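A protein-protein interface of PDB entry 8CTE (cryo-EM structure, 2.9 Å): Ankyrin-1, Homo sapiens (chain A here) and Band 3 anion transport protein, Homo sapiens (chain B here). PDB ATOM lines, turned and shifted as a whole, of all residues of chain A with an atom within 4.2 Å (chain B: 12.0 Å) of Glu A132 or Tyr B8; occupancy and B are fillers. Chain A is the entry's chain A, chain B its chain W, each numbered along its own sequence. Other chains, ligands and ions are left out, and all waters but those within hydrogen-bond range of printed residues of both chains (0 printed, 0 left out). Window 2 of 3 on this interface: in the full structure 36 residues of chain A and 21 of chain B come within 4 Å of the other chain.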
ATOM      1  N   LYS A 128      16.939   6.140   3.508  1.00  0.00           N
ATOM      2  CA  LYS A 128      18.355   6.444   3.323  1.00  0.00           C
ATOM      3  C   LYS A 128      18.999   5.499   2.319  1.00  0.00           C
ATOM      4  O   LYS A 128      19.738   5.936   1.427  1.00  0.00           O
ATOM      5  CB  LYS A 128      19.087   6.361   4.662  1.00  0.00           C
ATOM      6  CG  LYS A 128      18.737   7.452   5.655  1.00  0.00           C
ATOM      7  CD  LYS A 128      19.261   7.118   7.044  1.00  0.00           C
ATOM      8  CE  LYS A 128      20.738   6.755   7.010  1.00  0.00           C
ATOM      9  NZ  LYS A 128      21.573   7.860   6.465  1.00  0.00           N
ATOM     10  N   PHE A 129      18.723   4.198   2.443  1.00  0.00           N
ATOM     11  CA  PHE A 129      19.340   3.231   1.541  1.00  0.00           C
ATOM     12  C   PHE A 129      18.849   3.412   0.110  1.00  0.00           C
ATOM     13  O   PHE A 129      19.636   3.313  -0.838  1.00  0.00           O
ATOM     14  CB  PHE A 129      19.074   1.807   2.025  1.00  0.00           C
ATOM     15  CG  PHE A 129      19.814   0.762   1.243  1.00  0.00           C
ATOM     16  CD1 PHE A 129      21.157   0.520   1.485  1.00  0.00           C
ATOM     17  CD2 PHE A 129      19.174   0.030   0.260  1.00  0.00           C
ATOM     18  CE1 PHE A 129      21.844  -0.438   0.762  1.00  0.00           C
ATOM     19  CE2 PHE A 129      19.854  -0.927  -0.465  1.00  0.00           C
ATOM     20  CZ  PHE A 129      21.191  -1.163  -0.214  1.00  0.00           C
ATOM     21  N   LEU A 130      17.552   3.673  -0.069  1.00  0.00           N
ATOM     22  CA  LEU A 130      17.020   3.878  -1.414  1.00  0.00           C
ATOM     23  C   LEU A 130      17.563   5.158  -2.039  1.00  0.00           C
ATOM     24  O   LEU A 130      17.901   5.174  -3.229  1.00  0.00           O
ATOM     25  CB  LEU A 130      15.493   3.894  -1.378  1.00  0.00           C
ATOM     26  CG  LEU A 130      14.828   2.541  -1.117  1.00  0.00           C
ATOM     27  CD1 LEU A 130      13.325   2.692  -0.985  1.00  0.00           C
ATOM     28  CD2 LEU A 130      15.175   1.555  -2.220  1.00  0.00           C
ATOM     29  N   LEU A 131      17.660   6.237  -1.258  1.00  0.00           N
ATOM     30  CA  LEU A 131      18.216   7.480  -1.785  1.00  0.00           C
ATOM     31  C   LEU A 131      19.684   7.317  -2.152  1.00  0.00           C
ATOM     32  O   LEU A 131      20.141   7.858  -3.167  1.00  0.00           O
ATOM     33  CB  LEU A 131      18.037   8.608  -0.771  1.00  0.00           C
ATOM     34  CG  LEU A 131      16.627   9.186  -0.645  1.00  0.00           C
ATOM     35  CD1 LEU A 131      16.562  10.188   0.493  1.00  0.00           C
ATOM     36  CD2 LEU A 131      16.199   9.830  -1.953  1.00  0.00           C
ATOM     37  N   GLU A 132      20.443   6.575  -1.342  1.00  0.00           N
ATOM     38  CA  GLU A 132      21.843   6.331  -1.671  1.00  0.00           C
ATOM     39  C   GLU A 132      21.978   5.426  -2.890  1.00  0.00           C
ATOM     40  O   GLU A 132      23.014   5.434  -3.565  1.00  0.00           O
ATOM     41  CB  GLU A 132      22.567   5.724  -0.469  1.00  0.00           C
ATOM     42  CG  GLU A 132      22.803   6.697   0.673  1.00  0.00           C
ATOM     43  CD  GLU A 132      23.485   6.046   1.858  1.00  0.00           C
ATOM     44  OE1 GLU A 132      23.582   4.800   1.876  1.00  0.00           O
ATOM     45  OE2 GLU A 132      23.927   6.776   2.768  1.00  0.00           O
ATOM     46  N   ASN A 133      20.945   4.641  -3.191  1.00  0.00           N
ATOM     47  CA  ASN A 133      20.989   3.714  -4.315  1.00  0.00           C
ATOM     48  C   ASN A 133      20.312   4.252  -5.571  1.00  0.00           C
ATOM     49  O   ASN A 133      20.159   3.499  -6.538  1.00  0.00           O
ATOM     50  CB  ASN A 133      20.365   2.373  -3.918  1.00  0.00           C
ATOM     51  CG  ASN A 133      21.269   1.564  -3.008  1.00  0.00           C
ATOM     52  OD1 ASN A 133      22.065   0.750  -3.471  1.00  0.00           O
ATOM     53  ND2 ASN A 133      21.155   1.789  -1.705  1.00  0.00           N
ATOM     54  N   GLY A 134      19.904   5.518  -5.588  1.00  0.00           N
ATOM     55  CA  GLY A 134      19.401   6.142  -6.794  1.00  0.00           C
ATOM     56  C   GLY A 134      17.900   6.317  -6.894  1.00  0.00           C
ATOM     57  O   GLY A 134      17.405   6.588  -7.995  1.00  0.00           O
ATOM     58  N   TYR A 166      19.002  15.515   1.431  1.00  0.00           N
ATOM     59  CA  TYR A 166      19.589  14.732   0.349  1.00  0.00           C
ATOM     60  C   TYR A 166      19.343  15.393  -1.002  1.00  0.00           C
ATOM     61  O   TYR A 166      20.274  15.562  -1.800  1.00  0.00           O
ATOM     62  CB  TYR A 166      19.024  13.310   0.366  1.00  0.00           C
ATOM     63  CG  TYR A 166      19.815  12.321  -0.460  1.00  0.00           C
ATOM     64  CD1 TYR A 166      19.532  12.122  -1.805  1.00  0.00           C
ATOM     65  CD2 TYR A 166      20.846  11.581   0.107  1.00  0.00           C
ATOM     66  CE1 TYR A 166      20.253  11.217  -2.562  1.00  0.00           C
ATOM     67  CE2 TYR A 166      21.572  10.674  -0.642  1.00  0.00           C
ATOM     68  CZ  TYR A 166      21.271  10.497  -1.975  1.00  0.00           C
ATOM     69  OH  TYR A 166      21.992   9.595  -2.724  1.00  0.00           O
ATOM     70  N   LYS A 171      23.030   8.744  -7.263  1.00  0.00           N
ATOM     71  CA  LYS A 171      23.606   7.439  -6.958  1.00  0.00           C
ATOM     72  C   LYS A 171      25.011   7.615  -6.396  1.00  0.00           C
ATOM     73  O   LYS A 171      25.944   7.953  -7.131  1.00  0.00           O
ATOM     74  CB  LYS A 171      23.623   6.578  -8.218  1.00  0.00           C
ATOM     75  CG  LYS A 171      24.228   5.196  -8.041  1.00  0.00           C
ATOM     76  CD  LYS A 171      23.450   4.378  -7.029  1.00  0.00           C
ATOM     77  CE  LYS A 171      23.767   2.897  -7.151  1.00  0.00           C
ATOM     78  NZ  LYS A 171      23.363   2.353  -8.477  1.00  0.00           N
ATOM     79  N   VAL A 172      25.165   7.385  -5.093  1.00  0.00           N
ATOM     80  CA  VAL A 172      26.469   7.484  -4.446  1.00  0.00           C
ATOM     81  C   VAL A 172      27.041   6.087  -4.253  1.00  0.00           C
ATOM     82  O   VAL A 172      28.249   5.919  -4.058  1.00  0.00           O
ATOM     83  CB  VAL A 172      26.375   8.238  -3.106  1.00  0.00           C
ATOM     84  CG1 VAL A 172      25.951   9.681  -3.340  1.00  0.00           C
ATOM     85  CG2 VAL A 172      25.401   7.542  -2.171  1.00  0.00           C
ATOM     86  N   ARG A 173      26.177   5.077  -4.309  1.00  0.00           N
ATOM     87  CA  ARG A 173      26.626   3.697  -4.210  1.00  0.00           C
ATOM     88  C   ARG A 173      27.177   3.210  -5.545  1.00  0.00           C
ATOM     89  O   ARG A 173      26.880   3.761  -6.609  1.00  0.00           O
ATOM     90  CB  ARG A 173      25.481   2.788  -3.762  1.00  0.00           C
ATOM     91  CG  ARG A 173      25.190   2.825  -2.273  1.00  0.00           C
ATOM     92  CD  ARG A 173      25.284   1.432  -1.670  1.00  0.00           C
ATOM     93  NE  ARG A 173      24.476   0.466  -2.404  1.00  0.00           N
ATOM     94  CZ  ARG A 173      24.423  -0.830  -2.130  1.00  0.00           C
ATOM     95  NH1 ARG A 173      25.122  -1.357  -1.139  1.00  0.00           N
ATOM     96  NH2 ARG A 173      23.648  -1.619  -2.870  1.00  0.00           N
ATOM     97  N   LEU A 174      27.994   2.163  -5.477  1.00  0.00           N
ATOM     98  CA  LEU A 174      28.467   1.507  -6.682  1.00  0.00           C
ATOM     99  C   LEU A 174      27.332   0.720  -7.333  1.00  0.00           C
ATOM    100  O   LEU A 174      26.343   0.382  -6.676  1.00  0.00           O
ATOM    101  CB  LEU A 174      29.624   0.564  -6.361  1.00  0.00           C
ATOM    102  CG  LEU A 174      30.994   1.174  -6.081  1.00  0.00           C
ATOM    103  CD1 LEU A 174      31.982   0.080  -5.728  1.00  0.00           C
ATOM    104  CD2 LEU A 174      31.479   1.959  -7.285  1.00  0.00           C
ATOM    105  N   GLU B   2      30.022   0.135  10.399  1.00  0.00           N
ATOM    106  CA  GLU B   2      30.242   0.420   8.986  1.00  0.00           C
ATOM    107  C   GLU B   2      30.475  -0.865   8.198  1.00  0.00           C
ATOM    108  O   GLU B   2      29.531  -1.605   7.914  1.00  0.00           O
ATOM    109  CB  GLU B   2      31.429   1.370   8.810  1.00  0.00           C
ATOM    110  N   GLU B   3      31.738  -1.106   7.837  1.00  0.00           N
ATOM    111  CA  GLU B   3      32.178  -2.292   7.099  1.00  0.00           C
ATOM    112  C   GLU B   3      31.510  -2.417   5.733  1.00  0.00           C
ATOM    113  O   GLU B   3      31.485  -3.504   5.148  1.00  0.00           O
ATOM    114  CB  GLU B   3      31.956  -3.573   7.914  1.00  0.00           C
ATOM    115  N   LEU B   4      30.964  -1.315   5.205  1.00  0.00           N
ATOM    116  CA  LEU B   4      30.339  -1.327   3.888  1.00  0.00           C
ATOM    117  C   LEU B   4      30.698  -0.089   3.074  1.00  0.00           C
ATOM    118  O   LEU B   4      29.967   0.258   2.137  1.00  0.00           O
ATOM    119  CB  LEU B   4      28.814  -1.443   4.003  1.00  0.00           C
ATOM    120  CG  LEU B   4      28.253  -2.802   4.428  1.00  0.00           C
ATOM    121  CD1 LEU B   4      26.742  -2.738   4.572  1.00  0.00           C
ATOM    122  CD2 LEU B   4      28.653  -3.879   3.433  1.00  0.00           C
ATOM    123  N   GLN B   5      31.797   0.590   3.411  1.00  0.00           N
ATOM    124  CA  GLN B   5      32.206   1.774   2.667  1.00  0.00           C
ATOM    125  C   GLN B   5      32.640   1.444   1.245  1.00  0.00           C
ATOM    126  O   GLN B   5      32.546   2.308   0.368  1.00  0.00           O
ATOM    127  CB  GLN B   5      33.338   2.493   3.402  1.00  0.00           C
ATOM    128  N   ASP B   6      33.091   0.213   0.995  1.00  0.00           N
ATOM    129  CA  ASP B   6      33.550  -0.181  -0.332  1.00  0.00           C
ATOM    130  C   ASP B   6      32.427  -0.229  -1.360  1.00  0.00           C
ATOM    131  O   ASP B   6      32.714  -0.337  -2.556  1.00  0.00           O
ATOM    132  CB  ASP B   6      34.244  -1.542  -0.263  1.00  0.00           C
ATOM    133  N   ASP B   7      31.167  -0.155  -0.930  1.00  0.00           N
ATOM    134  CA  ASP B   7      30.040  -0.146  -1.852  1.00  0.00           C
ATOM    135  C   ASP B   7      29.747   1.237  -2.418  1.00  0.00           C
ATOM    136  O   ASP B   7      28.844   1.367  -3.251  1.00  0.00           O
ATOM    137  CB  ASP B   7      28.789  -0.687  -1.155  1.00  0.00           C
ATOM    138  CG  ASP B   7      29.003  -2.063  -0.556  1.00  0.00           C
ATOM    139  OD1 ASP B   7      30.127  -2.595  -0.670  1.00  0.00           O
ATOM    140  OD2 ASP B   7      28.047  -2.614   0.030  1.00  0.00           O
ATOM    141  N   TYR B   8      30.479   2.263  -1.993  1.00  0.00           N
ATOM    142  CA  TYR B   8      30.250   3.629  -2.438  1.00  0.00           C
ATOM    143  C   TYR B   8      31.298   4.044  -3.464  1.00  0.00           C
ATOM    144  O   TYR B   8      32.385   3.466  -3.541  1.00  0.00           O
ATOM    145  CB  TYR B   8      30.265   4.594  -1.250  1.00  0.00           C
ATOM    146  CG  TYR B   8      29.140   4.357  -0.268  1.00  0.00           C
ATOM    147  CD1 TYR B   8      29.300   3.488   0.804  1.00  0.00           C
ATOM    148  CD2 TYR B   8      27.917   4.997  -0.415  1.00  0.00           C
ATOM    149  CE1 TYR B   8      28.273   3.266   1.704  1.00  0.00           C
ATOM    150  CE2 TYR B   8      26.885   4.783   0.480  1.00  0.00           C
ATOM    151  CZ  TYR B   8      27.068   3.916   1.537  1.00  0.00           C
ATOM    152  OH  TYR B   8      26.045   3.698   2.429  1.00  0.00           O
ATOM    153  N   GLU B   9      30.948   5.057  -4.261  1.00  0.00           N
ATOM    154  CA  GLU B   9      31.814   5.482  -5.359  1.00  0.00           C
ATOM    155  C   GLU B   9      33.113   6.099  -4.851  1.00  0.00           C
ATOM    156  O   GLU B   9      34.194   5.804  -5.375  1.00  0.00           O
ATOM    157  CB  GLU B   9      31.070   6.473  -6.255  1.00  0.00           C
ATOM    158  CG  GLU B   9      29.857   5.896  -6.969  1.00  0.00           C
ATOM    159  CD  GLU B   9      30.225   5.102  -8.207  1.00  0.00           C
ATOM    160  OE1 GLU B   9      31.410   5.125  -8.601  1.00  0.00           O
ATOM    161  OE2 GLU B   9      29.328   4.454  -8.788  1.00  0.00           O
ATOM    162  N   ASP B  10      33.029   6.963  -3.835  1.00  0.00           N
ATOM    163  CA  ASP B  10      34.205   7.710  -3.393  1.00  0.00           C
ATOM    164  C   ASP B  10      35.237   6.800  -2.736  1.00  0.00           C
ATOM    165  O   ASP B  10      36.437   6.909  -3.019  1.00  0.00           O
ATOM    166  CB  ASP B  10      33.786   8.825  -2.436  1.00  0.00           C
ATOM    167  CG  ASP B  10      32.892   9.855  -3.098  1.00  0.00           C
ATOM    168  OD1 ASP B  10      32.617   9.715  -4.308  1.00  0.00           O
ATOM    169  OD2 ASP B  10      32.463  10.805  -2.408  1.00  0.00           O
ATOM    170  N   MET B  11      34.793   5.904  -1.853  1.00  0.00           N
ATOM    171  CA  MET B  11      35.728   5.003  -1.185  1.00  0.00           C
ATOM    172  C   MET B  11      36.360   4.030  -2.173  1.00  0.00           C
ATOM    173  O   MET B  11      37.553   3.724  -2.072  1.00  0.00           O
ATOM    174  CB  MET B  11      35.020   4.250  -0.060  1.00  0.00           C
ATOM    175  CG  MET B  11      35.922   3.318   0.731  1.00  0.00           C
ATOM    176  SD  MET B  11      37.313   4.176   1.492  1.00  0.00           S
ATOM    177  CE  MET B  11      36.455   5.353   2.534  1.00  0.00           C
ATOM    178  N   MET B  12      35.580   3.536  -3.136  1.00  0.00           N
ATOM    179  CA  MET B  12      36.141   2.665  -4.165  1.00  0.00           C
ATOM    180  C   MET B  12      37.150   3.411  -5.030  1.00  0.00           C
ATOM    181  O   MET B  12      38.188   2.852  -5.401  1.00  0.00           O
ATOM    182  CB  MET B  12      35.024   2.077  -5.026  1.00  0.00           C
ATOM    183  CG  MET B  12      35.518   1.141  -6.119  1.00  0.00           C
ATOM    184  SD  MET B  12      36.549  -0.190  -5.475  1.00  0.00           S
ATOM    185  CE  MET B  12      35.389  -1.039  -4.407  1.00  0.00           C
ATOM    186  N   GLU B  13      36.860   4.672  -5.362  1.00  0.00           N
ATOM    187  CA  GLU B  13      37.807   5.477  -6.128  1.00  0.00           C
ATOM    188  C   GLU B  13      39.099   5.692  -5.351  1.00  0.00           C
ATOM    189  O   GLU B  13      40.193   5.653  -5.928  1.00  0.00           O
ATOM    190  CB  GLU B  13      37.171   6.818  -6.497  1.00  0.00           C
ATOM    191  CG  GLU B  13      38.055   7.720  -7.342  1.00  0.00           C
ATOM    192  CD  GLU B  13      37.381   9.033  -7.691  1.00  0.00           C
ATOM    193  OE1 GLU B  13      36.225   9.240  -7.262  1.00  0.00           O
ATOM    194  OE2 GLU B  13      38.003   9.858  -8.393  1.00  0.00           O
ATOM    195  N   GLU B  14      38.992   5.928  -4.041  1.00  0.00           N
ATOM    196  CA  GLU B  14      40.185   6.060  -3.210  1.00  0.00           C
ATOM    197  C   GLU B  14      40.969   4.753  -3.150  1.00  0.00           C
ATOM    198  O   GLU B  14      42.205   4.759  -3.180  1.00  0.00           O
ATOM    199  CB  GLU B  14      39.796   6.517  -1.804  1.00  0.00           C
ATOM    200  CG  GLU B  14      39.318   7.957  -1.721  1.00  0.00           C
ATOM    201  CD  GLU B  14      40.450   8.960  -1.840  1.00  0.00           C
ATOM    202  OE1 GLU B  14      41.621   8.567  -1.651  1.00  0.00           O
ATOM    203  OE2 GLU B  14      40.168  10.144  -2.120  1.00  0.00           O
ATOM    204  N   ASN B  15      40.265   3.621  -3.058  1.00  0.00           N
ATOM    205  CA  ASN B  15      40.938   2.329  -2.958  1.00  0.00           C
ATOM    206  C   ASN B  15      41.644   1.961  -4.258  1.00  0.00           C
ATOM    207  O   ASN B  15      42.732   1.373  -4.233  1.00  0.00           O
ATOM    208  CB  ASN B  15      39.935   1.242  -2.571  1.00  0.00           C
ATOM    209  CG  ASN B  15      39.408   1.410  -1.161  1.00  0.00           C
ATOM    210  OD1 ASN B  15      40.107   1.911  -0.279  1.00  0.00           O
ATOM    211  ND2 ASN B  15      38.168   0.992  -0.940  1.00  0.00           N
ATOM    212  N   LEU B  16      41.039   2.290  -5.403  1.00  0.00           N
ATOM    213  CA  LEU B  16      41.627   1.916  -6.686  1.00  0.00           C
ATOM    214  C   LEU B  16      42.931   2.658  -6.954  1.00  0.00           C
ATOM    215  O   LEU B  16      43.782   2.154  -7.697  1.00  0.00           O
ATOM    216  CB  LEU B  16      40.624   2.163  -7.811  1.00  0.00           C
ATOM    217  CG  LEU B  16      39.467   1.163  -7.859  1.00  0.00           C
ATOM    218  CD1 LEU B  16      38.306   1.712  -8.666  1.00  0.00           C
ATOM    219  CD2 LEU B  16      39.934  -0.169  -8.427  1.00  0.00           C
ATOM    220  N   GLU B  17      43.103   3.842  -6.362  1.00  0.00           N
ATOM    221  CA  GLU B  17      44.348   4.612  -6.420  1.00  0.00           C
ATOM    222  C   GLU B  17      44.752   4.917  -7.864  1.00  0.00           C
ATOM    223  O   GLU B  17      45.776   4.452  -8.368  1.00  0.00           O
ATOM    224  CB  GLU B  17      45.472   3.890  -5.667  1.00  0.00           C
ATOM    225  CG  GLU B  17      45.209   3.722  -4.179  1.00  0.00           C
ATOM    226  CD  GLU B  17      46.354   3.041  -3.457  1.00  0.00           C
ATOM    227  OE1 GLU B  17      47.317   2.618  -4.130  1.00  0.00           O
ATOM    228  OE2 GLU B  17      46.292   2.929  -2.213  1.00  0.00           O
ATOM    229  N   GLN B  18      43.911   5.713  -8.529  1.00  0.00           N
ATOM    230  CA  GLN B  18      44.166   6.092  -9.913  1.00  0.00           C
ATOM    231  C   GLN B  18      45.406   6.966 -10.059  1.00  0.00           C
ATOM    232  O   GLN B  18      45.952   7.068 -11.163  1.00  0.00           O
ATOM    233  CB  GLN B  18      42.943   6.811 -10.483  1.00  0.00           C
ATOM    234  CG  GLN B  18      41.655   6.014 -10.349  1.00  0.00           C
ATOM    235  CD  GLN B  18      40.415   6.865 -10.541  1.00  0.00           C
ATOM    236  OE1 GLN B  18      39.296   6.418 -10.286  1.00  0.00           O
ATOM    237  NE2 GLN B  18      40.607   8.099 -10.991  1.00  0.00           N
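Of chain B, only Tyr B8 comes within 4 Å of Glu A132. Tyr B8 touches just these residues of chain A: Glu A132, Val A172, Arg A173 and Leu A174. No residue of chain B comes within 4 Å of Phe A129. No residue of chain B comes within 4 Å of Asn A133. No residue of chain B comes within 4 Å of Lys A171. Val A172 touches two residues of chain B. Of chain B, only Asp B7, Tyr B8 and Glu B9 come within 4 Å of Arg A173. Leu A174 touches just these residues of chain B: Asp B6 (3.3 Å), Asp B7 (2.5 Å), Tyr B8 (3.7 Å), Glu B9 (3.4 Å) and Met B12 (3.7 Å). Of the printed residues of chain A, Met B12 touches Leu A174 (3.7 Å). Of the printed residues of chain A, Asp B7 touches Arg A173 and Leu A174. Of the printed residues of chain A, Asp B6 touches Leu A174. Printed residues of chain A within 4 Å of Glu B9: Val A172 (2.8 Å), Arg A173 (3.3 Å) and Leu A174 (3.4 Å). Glu B3 touches none of the printed residues of chain A. Glu B2 touches none of the printed residues of chain A. The nearest residue of chain B that does not touch Glu A132 is Asp B7 (7.1 Å).
The backbone carbonyl oxygen (O) of Glu A132 sits at hydrogen-bond distance from the backbone NH (N) of Val A172 (3.3 Å). O of Glu A132 lies within hydrogen-bond range of N of Arg A173 (3.3 Å). The side-chain amide oxygen (OD1) of Asn A133 lies within hydrogen-bond range of the guanidinium group (NE) of Arg A173 (2.7 Å).
The side-chain carboxylate of Glu A132 is in hydrogen-bond range of the side-chain hydroxyl of Tyr B8, at 2.8 Å. The backbone carbonyl oxygen of Val A172 sits at hydrogen-bond distance from the backbone NH of Glu B9 (2.8 Å). The side-chain carboxylate (OD2) of Asp B7 lies within salt-bridge range of the guanidinium group (NH1) of Arg A173 (3.4 Å). The backbone carbonyl oxygen of Asp B7 lies within hydrogen-bond range of the backbone NH of Leu A174, at 2.5 Å. The backbone carbonyl oxygen (O) of Arg A173 lies close to the side-chain carboxylate (OE2) of Glu B9.
Of the 17 printed residues of chain B, 5 touch a printed residue of chain A. Hydrophobic or aromatic side chains of chain B within 4 Å of the printed part of chain A: Tyr B8 and Met B12. Of the 12 printed residues of chain A, 4 touch a printed residue of chain B. Printed residues of chain A that touch a printed residue of chain B: Glu A132, Val A172, Arg A173 and Leu A174. Hydrophobic or aromatic side chains of chain A that line the printed part of chain B: Val A172 and Leu A174. Among the printed residues, 11 pairs touch across the chains. Among the printed residues, Asp or Glu carboxylates within 4 Å of a Lys or Arg side-chain nitrogen of the other chain: Arg A173 with Asp B7.
Among the printed residues, merely in contact across the chains: Leu A174 with Asp B6 (3.3 Å), Leu A174 with Glu B9 (3.4 Å), Val A172 with Tyr B8 (3.4 Å), Leu A174 with Tyr B8 (3.7 Å), Leu A174 with Met B12 (3.7 Å) and Arg A173 with Tyr B8 (3.8 Å).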
